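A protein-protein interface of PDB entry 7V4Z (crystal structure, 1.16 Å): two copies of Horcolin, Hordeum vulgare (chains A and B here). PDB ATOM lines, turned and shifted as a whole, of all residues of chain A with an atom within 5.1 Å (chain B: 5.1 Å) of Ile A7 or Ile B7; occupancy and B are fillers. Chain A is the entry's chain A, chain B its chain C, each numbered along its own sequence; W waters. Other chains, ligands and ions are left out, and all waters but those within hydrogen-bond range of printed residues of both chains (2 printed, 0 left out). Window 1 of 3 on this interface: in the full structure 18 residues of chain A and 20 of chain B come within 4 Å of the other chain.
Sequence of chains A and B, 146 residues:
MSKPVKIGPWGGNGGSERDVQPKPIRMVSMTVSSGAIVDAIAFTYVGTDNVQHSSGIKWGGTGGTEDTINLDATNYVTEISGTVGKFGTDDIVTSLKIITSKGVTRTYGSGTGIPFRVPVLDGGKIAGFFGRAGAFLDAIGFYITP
The backbone carbonyl oxygen (O) of Lys A6 lies within hydrogen-bond range of the backbone NH (N) of Leu B121 (2.9 Å). The backbone NH (N) of Gly A8 is in hydrogen-bond range of the backbone carbonyl oxygen (O) of Pro B119 (2.9 Å). N of Gly B8 is in hydrogen-bond range of O of Pro A119 (3.0 Å). The backbone carbonyl oxygen (O) of Lys B6 is in hydrogen-bond range of the backbone NH (N) of Leu A121 (2.9 Å).
N of Ile A144 lies within hydrogen-bond range of O of Val A5 (2.9 Å). The backbone carbonyl oxygen (O) of Phe A142 lies within hydrogen-bond range of the backbone NH (N) of Ile A7 (2.9 Å). N of Gly A141 is in hydrogen-bond range of O of Phe A130 (2.8 Å). The backbone NH of Ile B144 is in hydrogen-bond range of the backbone carbonyl oxygen of Val B5 (2.9 Å). N of Phe B142 lies within hydrogen-bond range of O of Ile B7 (2.9 Å). O of Phe B130 lies within hydrogen-bond range of N of Gly B141 (2.8 Å).
Val A5 touches Ile B144 (CG1 to O, 3.8 Å). Val B120 touches Lys A6 (CA to O, 3.7 Å). Ile A7 touches Ile B7. O of Pro B119 touches CA of Ile A7, at 3.2 Å. O of Pro A119 touches CA of Ile B7, 3.2 Å away. CA of Val A120 touches O of Lys B6, 3.7 Å away. Leu A121 touches Gly B8. Leu A121 touches Phe B130. Phe A130 touches Leu B121. CG1 of Val B5 touches CG2 of Ile A144, 3.6 Å away.
Ile A7 touches just these residues of chain B: Ile B7 (3.7 Å) and Pro B119 (3.2 Å). Of the printed residues of chain B, Pro A119 touches Ile B7 and Gly B8. Of the printed residues of chain B, Ile A144 touches Val B5 (3.6 Å). Printed residues of chain A within 4 Å of Gly B8: Pro A119 and Leu A121. Trp B10 touches none of the printed residues of chain A. Printed residues of chain A within 4 Å of Leu B121: Lys A6, Gly A8 and Phe A130. The nearest residue of chain B that does not touch Ile A7 is Ile B144 (4.1 Å).
Hydrophobic or aromatic side chains of chain A that line the printed part of chain B: Val A5, Ile A7, Pro A119, Leu A121, Phe A130 and Ile A144. Of the 14 printed residues of chain B, 9 touch a printed residue of chain A. Printed residues of chain B that touch a printed residue of chain A: Val B5, Lys B6, Ile B7, Gly B8, Pro B119, Val B120, Leu B121, Phe B130 and Ile B144. Hydrophobic or aromatic side chains of chain B that line the printed part of chain A: Val B5, Ile B7, Pro B119, Val B120, Leu B121 and Phe B130. Among the printed residues, 15 pairs touch across the chains. Among the printed residues, no Asp or Glu carboxylate lies within 4 Å of a Lys or Arg side-chain nitrogen of the other chain.
Val A5 touches Ile B144, and with the chains exchanged Ile A144 touches Val B5. Ile B7 touches its own counterpart, Ile A7. Gly A8 touches Pro B119, and with the chains exchanged Pro A119 touches Gly B8. Gly A8 touches Leu B121, and with the chains exchanged Leu A121 touches Gly B8. Of the 15 pairs that touch across the chains among the printed residues, 15 have their exchanged pair printed and touching as well.
Water W2 lies within hydrogen-bond range of O of Leu A121 (2.8 Å) and N of Lys B6 (2.8 Å). Water W1 bridges the backbone carbonyl oxygen of Leu B121 (2.8 Å) and the backbone NH of Lys A6 (2.9 Å).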
ATOM      1  N   VAL A   5      19.617  31.101   7.760  1.00  0.00           N
ATOM      2  CA  VAL A   5      21.087  31.005   7.813  1.00  0.00           C
ATOM      3  C   VAL A   5      21.571  30.708   6.408  1.00  0.00           C
ATOM      4  O   VAL A   5      20.877  30.044   5.629  1.00  0.00           O
ATOM      5  CB  VAL A   5      21.556  29.984   8.831  1.00  0.00           C
ATOM      6  CG1 VAL A   5      21.051  30.200  10.227  1.00  0.00           C
ATOM      7  CG2 VAL A   5      21.542  28.612   8.492  1.00  0.00           C
ATOM      8  N   LYS A   6      22.754  31.171   6.111  1.00  0.00           N
ATOM      9  CA  LYS A   6      23.396  31.009   4.795  1.00  0.00           C
ATOM     10  C   LYS A   6      24.748  30.323   5.029  1.00  0.00           C
ATOM     11  O   LYS A   6      25.597  30.870   5.717  1.00  0.00           O
ATOM     12  CB  LYS A   6      23.601  32.391   4.162  1.00  0.00           C
ATOM     13  CG  LYS A   6      24.099  32.324   2.745  1.00  0.00           C
ATOM     14  CD  LYS A   6      24.385  33.674   2.109  1.00  0.00           C
ATOM     15  CE  LYS A   6      24.751  33.562   0.648  1.00  0.00           C
ATOM     16  NZ  LYS A   6      25.052  34.883   0.038  1.00  0.00           N
ATOM     17  N   ILE A   7      24.874  29.103   4.473  1.00  0.00           N
ATOM     18  CA  ILE A   7      26.091  28.313   4.704  1.00  0.00           C
ATOM     19  C   ILE A   7      26.632  27.785   3.390  1.00  0.00           C
ATOM     20  O   ILE A   7      25.874  27.496   2.447  1.00  0.00           O
ATOM     21  CB  ILE A   7      25.862  27.173   5.721  1.00  0.00           C
ATOM     22  CG1 ILE A   7      24.896  26.114   5.229  1.00  0.00           C
ATOM     23  CG2 ILE A   7      25.530  27.716   7.092  1.00  0.00           C
ATOM     24  CD1 ILE A   7      24.845  24.864   6.138  1.00  0.00           C
ATOM     25  N   GLY A   8      27.924  27.650   3.329  1.00  0.00           N
ATOM     26  CA  GLY A   8      28.608  27.122   2.150  1.00  0.00           C
ATOM     27  C   GLY A   8      29.434  28.202   1.473  1.00  0.00           C
ATOM     28  O   GLY A   8      29.841  29.159   2.106  1.00  0.00           O
ATOM     29  N   PRO A   9      29.712  28.050   0.170  1.00  0.00           N
ATOM     30  CA  PRO A   9      29.327  26.937  -0.682  1.00  0.00           C
ATOM     31  C   PRO A   9      30.347  25.802  -0.665  1.00  0.00           C
ATOM     32  O   PRO A   9      31.421  25.943  -0.089  1.00  0.00           O
ATOM     33  CB  PRO A   9      29.203  27.624  -2.029  1.00  0.00           C
ATOM     34  CG  PRO A   9      30.342  28.532  -2.027  1.00  0.00           C
ATOM     35  CD  PRO A   9      30.466  29.059  -0.597  1.00  0.00           C
ATOM     36  N   TRP A  10      29.986  24.705  -1.280  1.00  0.00           N
ATOM     37  CA  TRP A  10      30.860  23.533  -1.536  1.00  0.00           C
ATOM     38  C   TRP A  10      31.051  23.459  -3.043  1.00  0.00           C
ATOM     39  O   TRP A  10      30.062  23.450  -3.802  1.00  0.00           O
ATOM     40  CB  TRP A  10      30.170  22.271  -1.011  1.00  0.00           C
ATOM     41  CG  TRP A  10      30.075  22.250   0.484  1.00  0.00           C
ATOM     42  CD1 TRP A  10      30.983  21.705   1.355  1.00  0.00           C
ATOM     43  CD2 TRP A  10      29.075  22.861   1.295  1.00  0.00           C
ATOM     44  NE1 TRP A  10      30.617  21.957   2.638  1.00  0.00           N
ATOM     45  CE2 TRP A  10      29.453  22.661   2.656  1.00  0.00           C
ATOM     46  CE3 TRP A  10      27.893  23.548   1.047  1.00  0.00           C
ATOM     47  CZ2 TRP A  10      28.722  23.176   3.725  1.00  0.00           C
ATOM     48  CZ3 TRP A  10      27.161  24.013   2.119  1.00  0.00           C
ATOM     49  CH2 TRP A  10      27.562  23.840   3.428  1.00  0.00           C
ATOM     50  N   VAL A 118      24.926  17.899   4.188  1.00  0.00           N
ATOM     51  CA  VAL A 118      24.283  18.841   5.127  1.00  0.00           C
ATOM     52  C   VAL A 118      22.946  18.244   5.543  1.00  0.00           C
ATOM     53  O   VAL A 118      21.937  18.449   4.836  1.00  0.00           O
ATOM     54  CB  VAL A 118      24.137  20.215   4.483  1.00  0.00           C
ATOM     55  CG1 VAL A 118      23.408  21.146   5.441  1.00  0.00           C
ATOM     56  CG2 VAL A 118      25.481  20.790   4.070  1.00  0.00           C
ATOM     57  N   PRO A 119      22.917  17.509   6.642  1.00  0.00           N
ATOM     58  CA  PRO A 119      21.675  16.956   7.191  1.00  0.00           C
ATOM     59  C   PRO A 119      21.075  18.005   8.090  1.00  0.00           C
ATOM     60  O   PRO A 119      21.754  18.419   9.043  1.00  0.00           O
ATOM     61  CB  PRO A 119      22.104  15.715   7.968  1.00  0.00           C
ATOM     62  CG  PRO A 119      23.573  15.657   7.900  1.00  0.00           C
ATOM     63  CD  PRO A 119      24.071  16.979   7.402  1.00  0.00           C
ATOM     64  N   VAL A 120      19.820  18.377   7.912  1.00  0.00           N
ATOM     65  CA  VAL A 120      19.147  19.401   8.737  1.00  0.00           C
ATOM     66  C   VAL A 120      18.177  18.677   9.640  1.00  0.00           C
ATOM     67  O   VAL A 120      17.349  17.836   9.170  1.00  0.00           O
ATOM     68  CB  VAL A 120      18.441  20.427   7.863  1.00  0.00           C
ATOM     69  CG1 VAL A 120      17.923  21.528   8.756  1.00  0.00           C
ATOM     70  CG2 VAL A 120      19.376  20.984   6.830  1.00  0.00           C
ATOM     71  N   LEU A 121      18.259  18.962  10.919  1.00  0.00           N
ATOM     72  CA  LEU A 121      17.532  18.214  11.937  1.00  0.00           C
ATOM     73  C   LEU A 121      16.417  19.085  12.545  1.00  0.00           C
ATOM     74  O   LEU A 121      16.348  20.304  12.351  1.00  0.00           O
ATOM     75  CB  LEU A 121      18.498  17.774  13.039  1.00  0.00           C
ATOM     76  CG  LEU A 121      19.705  16.960  12.591  1.00  0.00           C
ATOM     77  CD1 LEU A 121      20.581  16.566  13.763  1.00  0.00           C
ATOM     78  CD2 LEU A 121      19.354  15.729  11.769  1.00  0.00           C
ATOM     79  N   PHE A 130      22.381  29.304  -3.183  1.00  0.00           N
ATOM     80  CA  PHE A 130      23.278  30.285  -3.823  1.00  0.00           C
ATOM     81  C   PHE A 130      24.448  29.498  -4.366  1.00  0.00           C
ATOM     82  O   PHE A 130      24.588  28.289  -4.043  1.00  0.00           O
ATOM     83  CB  PHE A 130      23.702  31.394  -2.851  1.00  0.00           C
ATOM     84  CG  PHE A 130      24.606  30.935  -1.739  1.00  0.00           C
ATOM     85  CD1 PHE A 130      24.090  30.333  -0.587  1.00  0.00           C
ATOM     86  CD2 PHE A 130      25.988  31.054  -1.848  1.00  0.00           C
ATOM     87  CE1 PHE A 130      24.943  29.883   0.420  1.00  0.00           C
ATOM     88  CE2 PHE A 130      26.840  30.618  -0.822  1.00  0.00           C
ATOM     89  CZ  PHE A 130      26.294  30.040   0.294  1.00  0.00           C
ATOM     90  N   GLY A 141      25.643  26.405  -2.265  1.00  0.00           N
ATOM     91  CA  GLY A 141      25.421  26.651  -0.851  1.00  0.00           C
ATOM     92  C   GLY A 141      23.926  26.746  -0.578  1.00  0.00           C
ATOM     93  O   GLY A 141      23.109  26.737  -1.504  1.00  0.00           O
ATOM     94  N   PHE A 142      23.593  26.809   0.709  1.00  0.00           N
ATOM     95  CA  PHE A 142      22.211  26.643   1.164  1.00  0.00           C
ATOM     96  C   PHE A 142      21.777  27.783   2.046  1.00  0.00           C
ATOM     97  O   PHE A 142      22.528  28.258   2.901  1.00  0.00           O
ATOM     98  CB  PHE A 142      22.032  25.321   1.933  1.00  0.00           C
ATOM     99  CG  PHE A 142      22.587  24.144   1.188  1.00  0.00           C
ATOM    100  CD1 PHE A 142      22.180  23.843  -0.080  1.00  0.00           C
ATOM    101  CD2 PHE A 142      23.655  23.414   1.677  1.00  0.00           C
ATOM    102  CE1 PHE A 142      22.762  22.816  -0.817  1.00  0.00           C
ATOM    103  CE2 PHE A 142      24.214  22.382   0.934  1.00  0.00           C
ATOM    104  CZ  PHE A 142      23.781  22.114  -0.324  1.00  0.00           C
ATOM    105  N   ILE A 144      18.936  28.013   5.011  1.00  0.00           N
ATOM    106  CA  ILE A 144      18.288  27.018   5.903  1.00  0.00           C
ATOM    107  C   ILE A 144      17.463  27.783   6.925  1.00  0.00           C
ATOM    108  O   ILE A 144      17.990  28.692   7.571  1.00  0.00           O
ATOM    109  CB  ILE A 144      19.324  26.095   6.556  1.00  0.00           C
ATOM    110  CG1 ILE A 144      20.271  25.523   5.529  1.00  0.00           C
ATOM    111  CG2 ILE A 144      18.627  25.002   7.369  1.00  0.00           C
ATOM    112  CD1 ILE A 144      21.292  24.567   6.067  1.00  0.00           C
ATOM    113  N   VAL B   5      19.312  26.804  13.738  1.00  0.00           N
ATOM    114  CA  VAL B   5      19.327  25.605  12.871  1.00  0.00           C
ATOM    115  C   VAL B   5      20.250  24.580  13.465  1.00  0.00           C
ATOM    116  O   VAL B   5      21.279  24.956  14.030  1.00  0.00           O
ATOM    117  CB  VAL B   5      19.682  26.051  11.461  1.00  0.00           C
ATOM    118  CG1 VAL B   5      20.275  25.014  10.589  1.00  0.00           C
ATOM    119  CG2 VAL B   5      18.699  26.953  10.816  1.00  0.00           C
ATOM    120  N   LYS B   6      19.940  23.313  13.275  1.00  0.00           N
ATOM    121  CA  LYS B   6      20.721  22.192  13.815  1.00  0.00           C
ATOM    122  C   LYS B   6      21.113  21.313  12.626  1.00  0.00           C
ATOM    123  O   LYS B   6      20.232  20.786  11.946  1.00  0.00           O
ATOM    124  CB  LYS B   6      19.883  21.403  14.818  1.00  0.00           C
ATOM    125  CG  LYS B   6      20.650  20.324  15.545  1.00  0.00           C
ATOM    126  CD  LYS B   6      19.834  19.466  16.490  1.00  0.00           C
ATOM    127  CE  LYS B   6      20.657  18.507  17.277  1.00  0.00           C
ATOM    128  NZ  LYS B   6      19.893  17.612  18.174  1.00  0.00           N
ATOM    129  N   ILE B   7      22.403  21.180  12.388  1.00  0.00           N
ATOM    130  CA  ILE B   7      22.908  20.405  11.244  1.00  0.00           C
ATOM    131  C   ILE B   7      23.995  19.456  11.661  1.00  0.00           C
ATOM    132  O   ILE B   7      24.793  19.712  12.559  1.00  0.00           O
ATOM    133  CB  ILE B   7      23.377  21.288  10.072  1.00  0.00           C
ATOM    134  CG1 ILE B   7      24.576  22.143  10.428  1.00  0.00           C
ATOM    135  CG2 ILE B   7      22.254  22.111   9.496  1.00  0.00           C
ATOM    136  CD1 ILE B   7      25.230  22.808   9.225  1.00  0.00           C
ATOM    137  N   GLY B   8      24.045  18.326  10.983  1.00  0.00           N
ATOM    138  CA  GLY B   8      25.064  17.304  11.228  1.00  0.00           C
ATOM    139  C   GLY B   8      24.431  16.044  11.806  1.00  0.00           C
ATOM    140  O   GLY B   8      23.269  15.794  11.595  1.00  0.00           O
ATOM    141  N   PRO B   9      25.201  15.258  12.600  1.00  0.00           N
ATOM    142  CA  PRO B   9      26.616  15.471  12.902  1.00  0.00           C
ATOM    143  C   PRO B   9      27.514  14.748  11.877  1.00  0.00           C
ATOM    144  O   PRO B   9      27.017  14.014  11.017  1.00  0.00           O
ATOM    145  CB  PRO B   9      26.765  14.809  14.263  1.00  0.00           C
ATOM    146  CG  PRO B   9      25.803  13.680  14.192  1.00  0.00           C
ATOM    147  CD  PRO B   9      24.675  14.076  13.254  1.00  0.00           C
ATOM    148  N   TRP B  10      28.793  15.015  11.987  1.00  0.00           N
ATOM    149  CA  TRP B  10      29.877  14.379  11.175  1.00  0.00           C
ATOM    150  C   TRP B  10      30.727  13.547  12.114  1.00  0.00           C
ATOM    151  O   TRP B  10      31.178  14.054  13.157  1.00  0.00           O
ATOM    152  CB  TRP B  10      30.686  15.435  10.454  1.00  0.00           C
ATOM    153  CG  TRP B  10      29.888  16.204   9.455  1.00  0.00           C
ATOM    154  CD1 TRP B  10      29.748  15.933   8.128  1.00  0.00           C
ATOM    155  CD2 TRP B  10      29.083  17.351   9.704  1.00  0.00           C
ATOM    156  NE1 TRP B  10      28.850  16.790   7.572  1.00  0.00           N
ATOM    157  CE2 TRP B  10      28.456  17.702   8.500  1.00  0.00           C
ATOM    158  CE3 TRP B  10      28.819  18.160  10.815  1.00  0.00           C
ATOM    159  CZ2 TRP B  10      27.601  18.790   8.388  1.00  0.00           C
ATOM    160  CZ3 TRP B  10      27.943  19.226  10.674  1.00  0.00           C
ATOM    161  CH2 TRP B  10      27.394  19.552   9.467  1.00  0.00           C
ATOM    162  N   VAL B 118      31.974  23.627   7.223  1.00  0.00           N
ATOM    163  CA  VAL B 118      30.759  24.447   7.312  1.00  0.00           C
ATOM    164  C   VAL B 118      31.159  25.905   7.461  1.00  0.00           C
ATOM    165  O   VAL B 118      31.395  26.336   8.614  1.00  0.00           O
ATOM    166  CB  VAL B 118      29.801  24.003   8.407  1.00  0.00           C
ATOM    167  CG1 VAL B 118      28.565  24.879   8.364  1.00  0.00           C
ATOM    168  CG2 VAL B 118      29.394  22.527   8.212  1.00  0.00           C
ATOM    169  N   PRO B 119      31.216  26.657   6.375  1.00  0.00           N
ATOM    170  CA  PRO B 119      31.402  28.104   6.464  1.00  0.00           C
ATOM    171  C   PRO B 119      30.057  28.774   6.613  1.00  0.00           C
ATOM    172  O   PRO B 119      29.064  28.424   5.910  1.00  0.00           O
ATOM    173  CB  PRO B 119      32.000  28.496   5.102  1.00  0.00           C
ATOM    174  CG  PRO B 119      32.012  27.219   4.268  1.00  0.00           C
ATOM    175  CD  PRO B 119      31.167  26.184   4.983  1.00  0.00           C
ATOM    176  N   VAL B 120      29.936  29.736   7.517  1.00  0.00           N
ATOM    177  CA  VAL B 120      28.692  30.486   7.778  1.00  0.00           C
ATOM    178  C   VAL B 120      28.860  31.896   7.294  1.00  0.00           C
ATOM    179  O   VAL B 120      29.913  32.553   7.635  1.00  0.00           O
ATOM    180  CB  VAL B 120      28.302  30.441   9.249  1.00  0.00           C
ATOM    181  CG1 VAL B 120      26.932  31.069   9.402  1.00  0.00           C
ATOM    182  CG2 VAL B 120      28.384  29.050   9.826  1.00  0.00           C
ATOM    183  N   LEU B 121      27.934  32.381   6.505  1.00  0.00           N
ATOM    184  CA  LEU B 121      28.111  33.698   5.864  1.00  0.00           C
ATOM    185  C   LEU B 121      27.154  34.757   6.435  1.00  0.00           C
ATOM    186  O   LEU B 121      26.234  34.455   7.239  1.00  0.00           O
ATOM    187  CB  LEU B 121      27.787  33.519   4.363  1.00  0.00           C
ATOM    188  CG  LEU B 121      28.674  32.522   3.623  1.00  0.00           C
ATOM    189  CD1 LEU B 121      28.295  32.429   2.163  1.00  0.00           C
ATOM    190  CD2 LEU B 121      30.160  32.931   3.779  1.00  0.00           C
ATOM    191  N   PHE B 130      26.404  19.744  19.269  1.00  0.00           N
ATOM    192  CA  PHE B 130      25.832  18.462  19.740  1.00  0.00           C
ATOM    193  C   PHE B 130      26.731  17.386  19.163  1.00  0.00           C
ATOM    194  O   PHE B 130      27.603  17.680  18.327  1.00  0.00           O
ATOM    195  CB  PHE B 130      24.374  18.254  19.329  1.00  0.00           C
ATOM    196  CG  PHE B 130      24.158  18.122  17.842  1.00  0.00           C
ATOM    197  CD1 PHE B 130      24.083  19.242  17.003  1.00  0.00           C
ATOM    198  CD2 PHE B 130      24.021  16.850  17.278  1.00  0.00           C
ATOM    199  CE1 PHE B 130      23.890  19.096  15.643  1.00  0.00           C
ATOM    200  CE2 PHE B 130      23.789  16.741  15.929  1.00  0.00           C
ATOM    201  CZ  PHE B 130      23.731  17.846  15.119  1.00  0.00           C
ATOM    202  N   GLY B 141      28.229  17.989  15.605  1.00  0.00           N
ATOM    203  CA  GLY B 141      27.284  18.772  14.814  1.00  0.00           C
ATOM    204  C   GLY B 141      27.156  20.171  15.385  1.00  0.00           C
ATOM    205  O   GLY B 141      27.671  20.452  16.458  1.00  0.00           O
ATOM    206  N   PHE B 142      26.467  21.021  14.605  1.00  0.00           N
ATOM    207  CA  PHE B 142      26.436  22.455  14.901  1.00  0.00           C
ATOM    208  C   PHE B 142      25.053  23.007  15.015  1.00  0.00           C
ATOM    209  O   PHE B 142      24.134  22.636  14.289  1.00  0.00           O
ATOM    210  CB  PHE B 142      27.154  23.232  13.775  1.00  0.00           C
ATOM    211  CG  PHE B 142      28.501  22.684  13.465  1.00  0.00           C
ATOM    212  CD1 PHE B 142      29.452  22.421  14.429  1.00  0.00           C
ATOM    213  CD2 PHE B 142      28.804  22.354  12.177  1.00  0.00           C
ATOM    214  CE1 PHE B 142      30.666  21.820  14.109  1.00  0.00           C
ATOM    215  CE2 PHE B 142      30.055  21.830  11.850  1.00  0.00           C
ATOM    216  CZ  PHE B 142      30.937  21.518  12.806  1.00  0.00           C
ATOM    217  N   ILE B 144      23.441  26.791  14.512  1.00  0.00           N
ATOM    218  CA  ILE B 144      23.865  27.986  13.737  1.00  0.00           C
ATOM    219  C   ILE B 144      22.745  29.007  13.827  1.00  0.00           C
ATOM    220  O   ILE B 144      21.543  28.671  13.631  1.00  0.00           O
ATOM    221  CB  ILE B 144      24.140  27.617  12.283  1.00  0.00           C
ATOM    222  CG1 ILE B 144      25.118  26.422  12.194  1.00  0.00           C
ATOM    223  CG2 ILE B 144      24.689  28.824  11.510  1.00  0.00           C
ATOM    224  CD1 ILE B 144      25.458  26.004  10.805  1.00  0.00           C
HETATM  225  O   HOH W   1      23.980  32.952   8.029  1.00  0.00           O
HETATM  226  O   HOH W   2      17.393  22.873  12.185  1.00  0.00           O
